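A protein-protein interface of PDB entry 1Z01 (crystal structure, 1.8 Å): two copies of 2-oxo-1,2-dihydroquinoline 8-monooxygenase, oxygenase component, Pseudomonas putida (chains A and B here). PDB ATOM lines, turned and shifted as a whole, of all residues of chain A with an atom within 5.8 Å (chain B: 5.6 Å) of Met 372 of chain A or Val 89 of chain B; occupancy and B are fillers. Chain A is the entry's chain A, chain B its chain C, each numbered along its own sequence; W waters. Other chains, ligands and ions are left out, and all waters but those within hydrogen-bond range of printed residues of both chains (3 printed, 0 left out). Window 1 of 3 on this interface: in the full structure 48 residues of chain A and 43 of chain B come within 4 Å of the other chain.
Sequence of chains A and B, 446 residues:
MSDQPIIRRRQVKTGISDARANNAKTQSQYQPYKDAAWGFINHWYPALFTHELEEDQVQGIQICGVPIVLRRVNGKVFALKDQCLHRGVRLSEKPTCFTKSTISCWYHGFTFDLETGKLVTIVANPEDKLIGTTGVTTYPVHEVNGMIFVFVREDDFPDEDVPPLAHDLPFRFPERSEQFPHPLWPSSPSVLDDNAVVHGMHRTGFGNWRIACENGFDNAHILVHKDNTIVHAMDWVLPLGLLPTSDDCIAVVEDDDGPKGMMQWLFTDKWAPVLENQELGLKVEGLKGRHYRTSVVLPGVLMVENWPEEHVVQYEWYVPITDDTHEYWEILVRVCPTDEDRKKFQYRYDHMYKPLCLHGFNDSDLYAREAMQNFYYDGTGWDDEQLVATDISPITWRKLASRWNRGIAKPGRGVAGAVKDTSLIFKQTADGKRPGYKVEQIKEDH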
ATOM      1  N   ILE A 211      -4.455 -11.021  35.337  1.00  0.00           N
ATOM      2  CA  ILE A 211      -3.981  -9.778  34.761  1.00  0.00           C
ATOM      3  C   ILE A 211      -5.113  -8.770  34.588  1.00  0.00           C
ATOM      4  O   ILE A 211      -4.901  -7.561  34.689  1.00  0.00           O
ATOM      5  CB  ILE A 211      -3.282 -10.062  33.424  1.00  0.00           C
ATOM      6  CG1 ILE A 211      -2.019 -10.894  33.693  1.00  0.00           C
ATOM      7  CG2 ILE A 211      -2.962  -8.768  32.705  1.00  0.00           C
ATOM      8  CD1 ILE A 211      -1.020 -10.226  34.655  1.00  0.00           C
ATOM      9  N   ALA A 212      -6.325  -9.258  34.344  1.00  0.00           N
ATOM     10  CA  ALA A 212      -7.463  -8.356  34.192  1.00  0.00           C
ATOM     11  C   ALA A 212      -7.886  -7.823  35.563  1.00  0.00           C
ATOM     12  O   ALA A 212      -8.245  -6.660  35.710  1.00  0.00           O
ATOM     13  CB  ALA A 212      -8.623  -9.085  33.544  1.00  0.00           C
ATOM     14  N   ASN A 215      -5.729  -4.665  37.500  1.00  0.00           N
ATOM     15  CA  ASN A 215      -5.846  -3.302  37.005  1.00  0.00           C
ATOM     16  C   ASN A 215      -6.819  -2.445  37.818  1.00  0.00           C
ATOM     17  O   ASN A 215      -6.526  -1.290  38.137  1.00  0.00           O
ATOM     18  CB  ASN A 215      -6.265  -3.340  35.529  1.00  0.00           C
ATOM     19  CG  ASN A 215      -6.792  -2.005  35.029  1.00  0.00           C
ATOM     20  OD1 ASN A 215      -7.969  -1.677  35.205  1.00  0.00           O
ATOM     21  ND2 ASN A 215      -5.923  -1.227  34.407  1.00  0.00           N
ATOM     22  N   TYR A 367      -8.959  -2.500  27.306  1.00  0.00           N
ATOM     23  CA  TYR A 367      -7.837  -2.651  26.391  1.00  0.00           C
ATOM     24  C   TYR A 367      -6.483  -2.608  27.097  1.00  0.00           C
ATOM     25  O   TYR A 367      -5.521  -3.228  26.643  1.00  0.00           O
ATOM     26  CB  TYR A 367      -7.918  -1.589  25.295  1.00  0.00           C
ATOM     27  CG  TYR A 367      -9.212  -1.671  24.520  1.00  0.00           C
ATOM     28  CD1 TYR A 367     -10.238  -0.752  24.734  1.00  0.00           C
ATOM     29  CD2 TYR A 367      -9.431  -2.705  23.609  1.00  0.00           C
ATOM     30  CE1 TYR A 367     -11.457  -0.860  24.059  1.00  0.00           C
ATOM     31  CE2 TYR A 367     -10.644  -2.826  22.928  1.00  0.00           C
ATOM     32  CZ  TYR A 367     -11.653  -1.902  23.156  1.00  0.00           C
ATOM     33  OH  TYR A 367     -12.850  -2.019  22.480  1.00  0.00           O
ATOM     34  N   ALA A 368      -6.401  -1.881  28.207  1.00  0.00           N
ATOM     35  CA  ALA A 368      -5.150  -1.809  28.957  1.00  0.00           C
ATOM     36  C   ALA A 368      -4.808  -3.200  29.484  1.00  0.00           C
ATOM     37  O   ALA A 368      -3.652  -3.617  29.438  1.00  0.00           O
ATOM     38  CB  ALA A 368      -5.285  -0.829  30.114  1.00  0.00           C
ATOM     39  N   ARG A 369      -5.822  -3.911  29.981  1.00  0.00           N
ATOM     40  CA  ARG A 369      -5.653  -5.267  30.509  1.00  0.00           C
ATOM     41  C   ARG A 369      -5.159  -6.216  29.434  1.00  0.00           C
ATOM     42  O   ARG A 369      -4.270  -7.028  29.673  1.00  0.00           O
ATOM     43  CB  ARG A 369      -6.979  -5.818  31.025  1.00  0.00           C
ATOM     44  CG  ARG A 369      -7.607  -5.057  32.152  1.00  0.00           C
ATOM     45  CD  ARG A 369      -9.023  -5.546  32.353  1.00  0.00           C
ATOM     46  NE  ARG A 369      -9.784  -4.641  33.205  1.00  0.00           N
ATOM     47  CZ  ARG A 369     -11.101  -4.493  33.141  1.00  0.00           C
ATOM     48  NH1 ARG A 369     -11.705  -3.644  33.959  1.00  0.00           N
ATOM     49  NH2 ARG A 369     -11.809  -5.188  32.256  1.00  0.00           N
ATOM     50  N   GLU A 370      -5.772  -6.131  28.258  1.00  0.00           N
ATOM     51  CA  GLU A 370      -5.405  -6.978  27.136  1.00  0.00           C
ATOM     52  C   GLU A 370      -3.957  -6.788  26.714  1.00  0.00           C
ATOM     53  O   GLU A 370      -3.235  -7.758  26.485  1.00  0.00           O
ATOM     54  CB  GLU A 370      -6.298  -6.674  25.936  1.00  0.00           C
ATOM     55  CG  GLU A 370      -7.477  -7.591  25.787  1.00  0.00           C
ATOM     56  CD  GLU A 370      -8.207  -7.372  24.480  1.00  0.00           C
ATOM     57  OE1 GLU A 370      -7.588  -6.833  23.544  1.00  0.00           O
ATOM     58  OE2 GLU A 370      -9.393  -7.753  24.383  1.00  0.00           O
ATOM     59  N   ALA A 371      -3.549  -5.529  26.594  1.00  0.00           N
ATOM     60  CA  ALA A 371      -2.191  -5.180  26.178  1.00  0.00           C
ATOM     61  C   ALA A 371      -1.084  -5.746  27.066  1.00  0.00           C
ATOM     62  O   ALA A 371       0.069  -5.842  26.649  1.00  0.00           O
ATOM     63  CB  ALA A 371      -2.063  -3.665  26.099  1.00  0.00           C
ATOM     64  N   MET A 372      -1.429  -6.122  28.286  1.00  0.00           N
ATOM     65  CA  MET A 372      -0.450  -6.655  29.222  1.00  0.00           C
ATOM     66  C   MET A 372      -0.389  -8.188  29.231  1.00  0.00           C
ATOM     67  O   MET A 372       0.576  -8.771  29.706  1.00  0.00           O
ATOM     68  CB  MET A 372      -0.787  -6.096  30.613  1.00  0.00           C
ATOM     69  CG  MET A 372      -0.079  -6.694  31.796  1.00  0.00           C
ATOM     70  SD  MET A 372      -0.399  -5.664  33.269  1.00  0.00           S
ATOM     71  CE  MET A 372      -2.183  -5.586  33.294  1.00  0.00           C
ATOM     72  N   GLN A 373      -1.405  -8.836  28.666  1.00  0.00           N
ATOM     73  CA  GLN A 373      -1.479 -10.302  28.660  1.00  0.00           C
ATOM     74  C   GLN A 373      -0.317 -11.072  28.015  1.00  0.00           C
ATOM     75  O   GLN A 373       0.105 -12.090  28.559  1.00  0.00           O
ATOM     76  CB  GLN A 373      -2.806 -10.755  28.033  1.00  0.00           C
ATOM     77  CG  GLN A 373      -4.059 -10.210  28.725  1.00  0.00           C
ATOM     78  CD  GLN A 373      -4.345 -10.861  30.074  1.00  0.00           C
ATOM     79  OE1 GLN A 373      -3.559 -11.662  30.581  1.00  0.00           O
ATOM     80  NE2 GLN A 373      -5.480 -10.515  30.661  1.00  0.00           N
ATOM     81  N   ASN A 374       0.205 -10.606  26.877  1.00  0.00           N
ATOM     82  CA  ASN A 374       1.316 -11.303  26.199  1.00  0.00           C
ATOM     83  C   ASN A 374       2.592 -11.448  27.023  1.00  0.00           C
ATOM     84  O   ASN A 374       3.329 -12.425  26.891  1.00  0.00           O
ATOM     85  CB  ASN A 374       1.674 -10.607  24.882  1.00  0.00           C
ATOM     86  CG  ASN A 374       0.737 -10.984  23.753  1.00  0.00           C
ATOM     87  OD1 ASN A 374       0.678 -10.301  22.727  1.00  0.00           O
ATOM     88  ND2 ASN A 374       0.007 -12.081  23.926  1.00  0.00           N
ATOM     89  N   PHE A 375       2.859 -10.468  27.867  1.00  0.00           N
ATOM     90  CA  PHE A 375       4.046 -10.483  28.704  1.00  0.00           C
ATOM     91  C   PHE A 375       3.986 -11.616  29.720  1.00  0.00           C
ATOM     92  O   PHE A 375       5.003 -12.210  30.063  1.00  0.00           O
ATOM     93  CB  PHE A 375       4.163  -9.130  29.429  1.00  0.00           C
ATOM     94  CG  PHE A 375       5.435  -8.950  30.219  1.00  0.00           C
ATOM     95  CD1 PHE A 375       6.671  -9.231  29.653  1.00  0.00           C
ATOM     96  CD2 PHE A 375       5.397  -8.414  31.509  1.00  0.00           C
ATOM     97  CE1 PHE A 375       7.850  -8.978  30.347  1.00  0.00           C
ATOM     98  CE2 PHE A 375       6.567  -8.156  32.211  1.00  0.00           C
ATOM     99  CZ  PHE A 375       7.800  -8.436  31.630  1.00  0.00           C
ATOM    100  N   TYR A 376       2.779 -11.931  30.176  1.00  0.00           N
ATOM    101  CA  TYR A 376       2.585 -12.945  31.201  1.00  0.00           C
ATOM    102  C   TYR A 376       2.182 -14.366  30.832  1.00  0.00           C
ATOM    103  O   TYR A 376       2.502 -15.294  31.579  1.00  0.00           O
ATOM    104  CB  TYR A 376       1.558 -12.434  32.213  1.00  0.00           C
ATOM    105  CG  TYR A 376       2.022 -11.245  33.010  1.00  0.00           C
ATOM    106  CD1 TYR A 376       2.653 -11.411  34.244  1.00  0.00           C
ATOM    107  CD2 TYR A 376       1.833  -9.949  32.528  1.00  0.00           C
ATOM    108  CE1 TYR A 376       3.081 -10.306  34.985  1.00  0.00           C
ATOM    109  CE2 TYR A 376       2.255  -8.844  33.254  1.00  0.00           C
ATOM    110  CZ  TYR A 376       2.874  -9.028  34.480  1.00  0.00           C
ATOM    111  OH  TYR A 376       3.286  -7.931  35.196  1.00  0.00           O
ATOM    112  N   ASP B  82       9.910  -2.150  21.968  1.00  0.00           N
ATOM    113  CA  ASP B  82       8.494  -1.865  22.192  1.00  0.00           C
ATOM    114  C   ASP B  82       7.965  -2.720  23.335  1.00  0.00           C
ATOM    115  O   ASP B  82       7.033  -3.510  23.159  1.00  0.00           O
ATOM    116  CB  ASP B  82       7.699  -2.149  20.909  1.00  0.00           C
ATOM    117  CG  ASP B  82       6.338  -1.492  20.914  1.00  0.00           C
ATOM    118  OD1 ASP B  82       5.530  -1.799  20.015  1.00  0.00           O
ATOM    119  OD2 ASP B  82       6.080  -0.665  21.822  1.00  0.00           O
ATOM    120  N   GLN B  83       8.575  -2.565  24.506  1.00  0.00           N
ATOM    121  CA  GLN B  83       8.171  -3.336  25.674  1.00  0.00           C
ATOM    122  C   GLN B  83       8.480  -2.602  26.969  1.00  0.00           C
ATOM    123  O   GLN B  83       9.636  -2.522  27.394  1.00  0.00           O
ATOM    124  CB  GLN B  83       8.888  -4.685  25.688  1.00  0.00           C
ATOM    125  CG  GLN B  83       8.511  -5.543  26.874  1.00  0.00           C
ATOM    126  CD  GLN B  83       9.475  -6.693  27.093  1.00  0.00           C
ATOM    127  OE1 GLN B  83      10.652  -6.477  27.377  1.00  0.00           O
ATOM    128  NE2 GLN B  83       8.977  -7.926  26.966  1.00  0.00           N
ATOM    129  N   CYS B  84       7.442  -2.074  27.601  1.00  0.00           N
ATOM    130  CA  CYS B  84       7.623  -1.365  28.852  1.00  0.00           C
ATOM    131  C   CYS B  84       8.250  -2.357  29.814  1.00  0.00           C
ATOM    132  O   CYS B  84       7.770  -3.480  29.933  1.00  0.00           O
ATOM    133  CB  CYS B  84       6.273  -0.896  29.387  1.00  0.00           C
ATOM    134  SG  CYS B  84       6.410   0.109  30.851  1.00  0.00           S
ATOM    135  N   ARG B  87       5.412  -3.633  33.206  1.00  0.00           N
ATOM    136  CA  ARG B  87       4.584  -4.820  33.061  1.00  0.00           C
ATOM    137  C   ARG B  87       4.383  -5.313  31.628  1.00  0.00           C
ATOM    138  O   ARG B  87       3.361  -5.918  31.288  1.00  0.00           O
ATOM    139  CB  ARG B  87       3.257  -4.618  33.793  1.00  0.00           C
ATOM    140  CG  ARG B  87       3.514  -4.338  35.274  1.00  0.00           C
ATOM    141  CD  ARG B  87       2.285  -4.424  36.148  1.00  0.00           C
ATOM    142  NE  ARG B  87       1.721  -5.768  36.148  1.00  0.00           N
ATOM    143  CZ  ARG B  87       0.701  -6.142  36.911  1.00  0.00           C
ATOM    144  NH1 ARG B  87       0.237  -7.385  36.848  1.00  0.00           N
ATOM    145  NH2 ARG B  87       0.153  -5.272  37.744  1.00  0.00           N
ATOM    146  N   GLY B  88       5.382  -5.036  30.796  1.00  0.00           N
ATOM    147  CA  GLY B  88       5.414  -5.515  29.425  1.00  0.00           C
ATOM    148  C   GLY B  88       4.429  -5.154  28.331  1.00  0.00           C
ATOM    149  O   GLY B  88       4.306  -5.921  27.376  1.00  0.00           O
ATOM    150  N   VAL B  89       3.726  -4.029  28.432  1.00  0.00           N
ATOM    151  CA  VAL B  89       2.808  -3.641  27.371  1.00  0.00           C
ATOM    152  C   VAL B  89       3.649  -2.986  26.277  1.00  0.00           C
ATOM    153  O   VAL B  89       4.784  -2.560  26.523  1.00  0.00           O
ATOM    154  CB  VAL B  89       1.769  -2.594  27.848  1.00  0.00           C
ATOM    155  CG1 VAL B  89       0.990  -3.109  29.055  1.00  0.00           C
ATOM    156  CG2 VAL B  89       2.467  -1.288  28.159  1.00  0.00           C
ATOM    157  N   ARG B  90       3.096  -2.904  25.073  1.00  0.00           N
ATOM    158  CA  ARG B  90       3.792  -2.261  23.964  1.00  0.00           C
ATOM    159  C   ARG B  90       3.578  -0.756  24.047  1.00  0.00           C
ATOM    160  O   ARG B  90       2.443  -0.274  24.093  1.00  0.00           O
ATOM    161  CB  ARG B  90       3.279  -2.785  22.613  1.00  0.00           C
ATOM    162  CG  ARG B  90       3.858  -4.133  22.214  1.00  0.00           C
ATOM    163  CD  ARG B  90       3.341  -4.610  20.867  1.00  0.00           C
ATOM    164  NE  ARG B  90       1.891  -4.792  20.863  1.00  0.00           N
ATOM    165  CZ  ARG B  90       1.240  -5.610  20.041  1.00  0.00           C
ATOM    166  NH1 ARG B  90      -0.082  -5.702  20.118  1.00  0.00           N
ATOM    167  NH2 ARG B  90       1.907  -6.338  19.148  1.00  0.00           N
ATOM    168  N   LEU B  91       4.678  -0.014  24.060  1.00  0.00           N
ATOM    169  CA  LEU B  91       4.619   1.440  24.147  1.00  0.00           C
ATOM    170  C   LEU B  91       3.875   2.051  22.958  1.00  0.00           C
ATOM    171  O   LEU B  91       3.184   3.058  23.094  1.00  0.00           O
ATOM    172  CB  LEU B  91       6.040   2.003  24.219  1.00  0.00           C
ATOM    173  CG  LEU B  91       6.884   1.528  25.411  1.00  0.00           C
ATOM    174  CD1 LEU B  91       8.322   1.954  25.220  1.00  0.00           C
ATOM    175  CD2 LEU B  91       6.328   2.098  26.706  1.00  0.00           C
ATOM    176  N   CYS B 105       5.099   5.223  28.758  1.00  0.00           N
ATOM    177  CA  CYS B 105       4.159   4.127  28.653  1.00  0.00           C
ATOM    178  C   CYS B 105       2.810   4.698  29.070  1.00  0.00           C
ATOM    179  O   CYS B 105       2.675   5.303  30.137  1.00  0.00           O
ATOM    180  CB  CYS B 105       4.539   2.974  29.576  1.00  0.00           C
ATOM    181  SG  CYS B 105       3.336   1.638  29.475  1.00  0.00           S
ATOM    182  N   TRP B 106       1.817   4.504  28.213  1.00  0.00           N
ATOM    183  CA  TRP B 106       0.468   5.000  28.430  1.00  0.00           C
ATOM    184  C   TRP B 106      -0.277   4.349  29.585  1.00  0.00           C
ATOM    185  O   TRP B 106      -1.377   4.784  29.943  1.00  0.00           O
ATOM    186  CB  TRP B 106      -0.343   4.783  27.161  1.00  0.00           C
ATOM    187  CG  TRP B 106      -0.185   3.384  26.633  1.00  0.00           C
ATOM    188  CD1 TRP B 106       0.765   2.934  25.749  1.00  0.00           C
ATOM    189  CD2 TRP B 106      -0.962   2.241  26.998  1.00  0.00           C
ATOM    190  NE1 TRP B 106       0.621   1.581  25.543  1.00  0.00           N
ATOM    191  CE2 TRP B 106      -0.430   1.131  26.299  1.00  0.00           C
ATOM    192  CE3 TRP B 106      -2.055   2.046  27.850  1.00  0.00           C
ATOM    193  CZ2 TRP B 106      -0.957  -0.154  26.427  1.00  0.00           C
ATOM    194  CZ3 TRP B 106      -2.580   0.766  27.979  1.00  0.00           C
ATOM    195  CH2 TRP B 106      -2.029  -0.319  27.268  1.00  0.00           C
ATOM    196  N   TYR B 107       0.309   3.312  30.165  1.00  0.00           N
ATOM    197  CA  TYR B 107      -0.356   2.599  31.240  1.00  0.00           C
ATOM    198  C   TYR B 107      -0.062   3.152  32.629  1.00  0.00           C
ATOM    199  O   TYR B 107      -0.972   3.665  33.283  1.00  0.00           O
ATOM    200  CB  TYR B 107       0.011   1.120  31.162  1.00  0.00           C
ATOM    201  CG  TYR B 107      -1.017   0.175  31.740  1.00  0.00           C
ATOM    202  CD1 TYR B 107      -0.947  -1.189  31.472  1.00  0.00           C
ATOM    203  CD2 TYR B 107      -2.058   0.635  32.551  1.00  0.00           C
ATOM    204  CE1 TYR B 107      -1.882  -2.074  31.990  1.00  0.00           C
ATOM    205  CE2 TYR B 107      -3.000  -0.244  33.077  1.00  0.00           C
ATOM    206  CZ  TYR B 107      -2.907  -1.597  32.791  1.00  0.00           C
ATOM    207  OH  TYR B 107      -3.847  -2.483  33.290  1.00  0.00           O
ATOM    208  N   HIS B 108       1.187   3.045  33.088  1.00  0.00           N
ATOM    209  CA  HIS B 108       1.545   3.552  34.416  1.00  0.00           C
ATOM    210  C   HIS B 108       2.602   4.651  34.366  1.00  0.00           C
ATOM    211  O   HIS B 108       3.176   5.018  35.390  1.00  0.00           O
ATOM    212  CB  HIS B 108       2.022   2.415  35.334  1.00  0.00           C
ATOM    213  CG  HIS B 108       1.067   1.264  35.422  1.00  0.00           C
ATOM    214  ND1 HIS B 108       1.178   0.143  34.630  1.00  0.00           N
ATOM    215  CD2 HIS B 108      -0.028   1.070  36.193  1.00  0.00           C
ATOM    216  CE1 HIS B 108       0.195  -0.695  34.911  1.00  0.00           C
ATOM    217  NE2 HIS B 108      -0.551  -0.155  35.856  1.00  0.00           N
HETATM  218  O   HOH W   1       2.030  -7.414  23.115  1.00  0.00           O
HETATM  219  O   HOH W   2       0.833  -4.717  24.556  1.00  0.00           O
HETATM  220  O   HOH W   3       2.169  -7.530  26.255  1.00  0.00           O
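The side-chain sulfur (SD) of Met 372 of chain A is in hydrogen-bond range of the guanidinium group (NE) of Arg 87 of chain B (3.6 Å). The guanidinium group (NE) of Arg 87 of chain B is in hydrogen-bond range of the side-chain hydroxyl (OH) of Tyr 376 of chain A (2.8 Å). The side-chain amide nitrogen (ND2) of Asn 215 of chain A is in hydrogen-bond range of the side-chain hydroxyl (OH) of Tyr 107 of chain B (2.7 Å).
The backbone carbonyl oxygen (O) of Val 89 of chain B lies within hydrogen-bond range of the backbone NH (N) of Cys 84 of chain B (2.9 Å). The indole nitrogen (NE1) of Trp 106 of chain B sits at hydrogen-bond distance from the backbone carbonyl oxygen (O) of Arg 90 of chain B, 3.0 Å away. The side-chain sulfur (SG) of Cys 105 of chain B sits close to the backbone NH (N) of Tyr 107 of chain B, 3.5 Å away.
NH1 of Arg 87 of chain B touches CD1 of Ile 211 of chain A, 3.8 Å away. Ala 368 of chain A touches Trp 106 of chain B (CA to CZ3, 3.8 Å). O of Ala 368 of chain A touches CE1 of Tyr 107 of chain B (3.5 Å). Ala 371 of chain A touches Val 89 of chain B. Ala 371 of chain A touches Trp 106 of chain B (CB to CH2, 3.5 Å). CB of Met 372 of chain A touches CG1 of Val 89 of chain B, 3.8 Å away. CE of Met 372 of chain A touches OH of Tyr 107 of chain B, 3.5 Å away. Phe 375 of chain A touches Gln 83 of chain B. Phe 375 of chain A touches Arg 87 of chain B (CD2 to O, 3.2 Å). Phe 375 of chain A touches Gly 88 of chain B (CD2 to N, 3.5 Å).
Of chain B, only Arg 87 (3.6 Å), Val 89 (3.8 Å) and Tyr 107 (3.5 Å) come within 4 Å of Met 372 of chain A. Of the printed residues of chain A, Tyr 107 of chain B touches Asn 215, Ala 368 and Met 372. Printed residues of chain A within 4 Å of Gln 83 of chain B: Phe 375 (3.7 Å). Asp 82 of chain B touches none of the printed residues of chain A. His 108 of chain B touches none of the printed residues of chain A. The nearest residue of chain B that does not touch Met 372 of chain A is Gly 88 of chain B (5.2 Å). The nearest printed residue of chain B that does not touch Ile 211 of chain A is Tyr 107 of chain B (5.4 Å).
Among the printed residues, 13 pairs touch across the chains. Among the printed residues, no Asp or Glu carboxylate lies within 4 Å of a Lys or Arg side-chain nitrogen of the other chain.
No position is printed for both chains. Of the 13 pairs that touch across the chains among the printed residues, none has its exchanged pair printed and touching as well.
Water W2 bridges the backbone carbonyl oxygen (O) of Ala 371 of chain A (2.5 Å) and the backbone NH (N) of Arg 90 of chain B (2.9 Å). Water W3 lies within hydrogen-bond range of O of Ala 371 of chain A (2.7 Å), O of Gly 88 of chain B (2.9 Å) and N of Phe 375 of chain A (3.4 Å). Water W1 bridges OD1 of Asn 374 of chain A and NE of Arg 90 of chain B.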
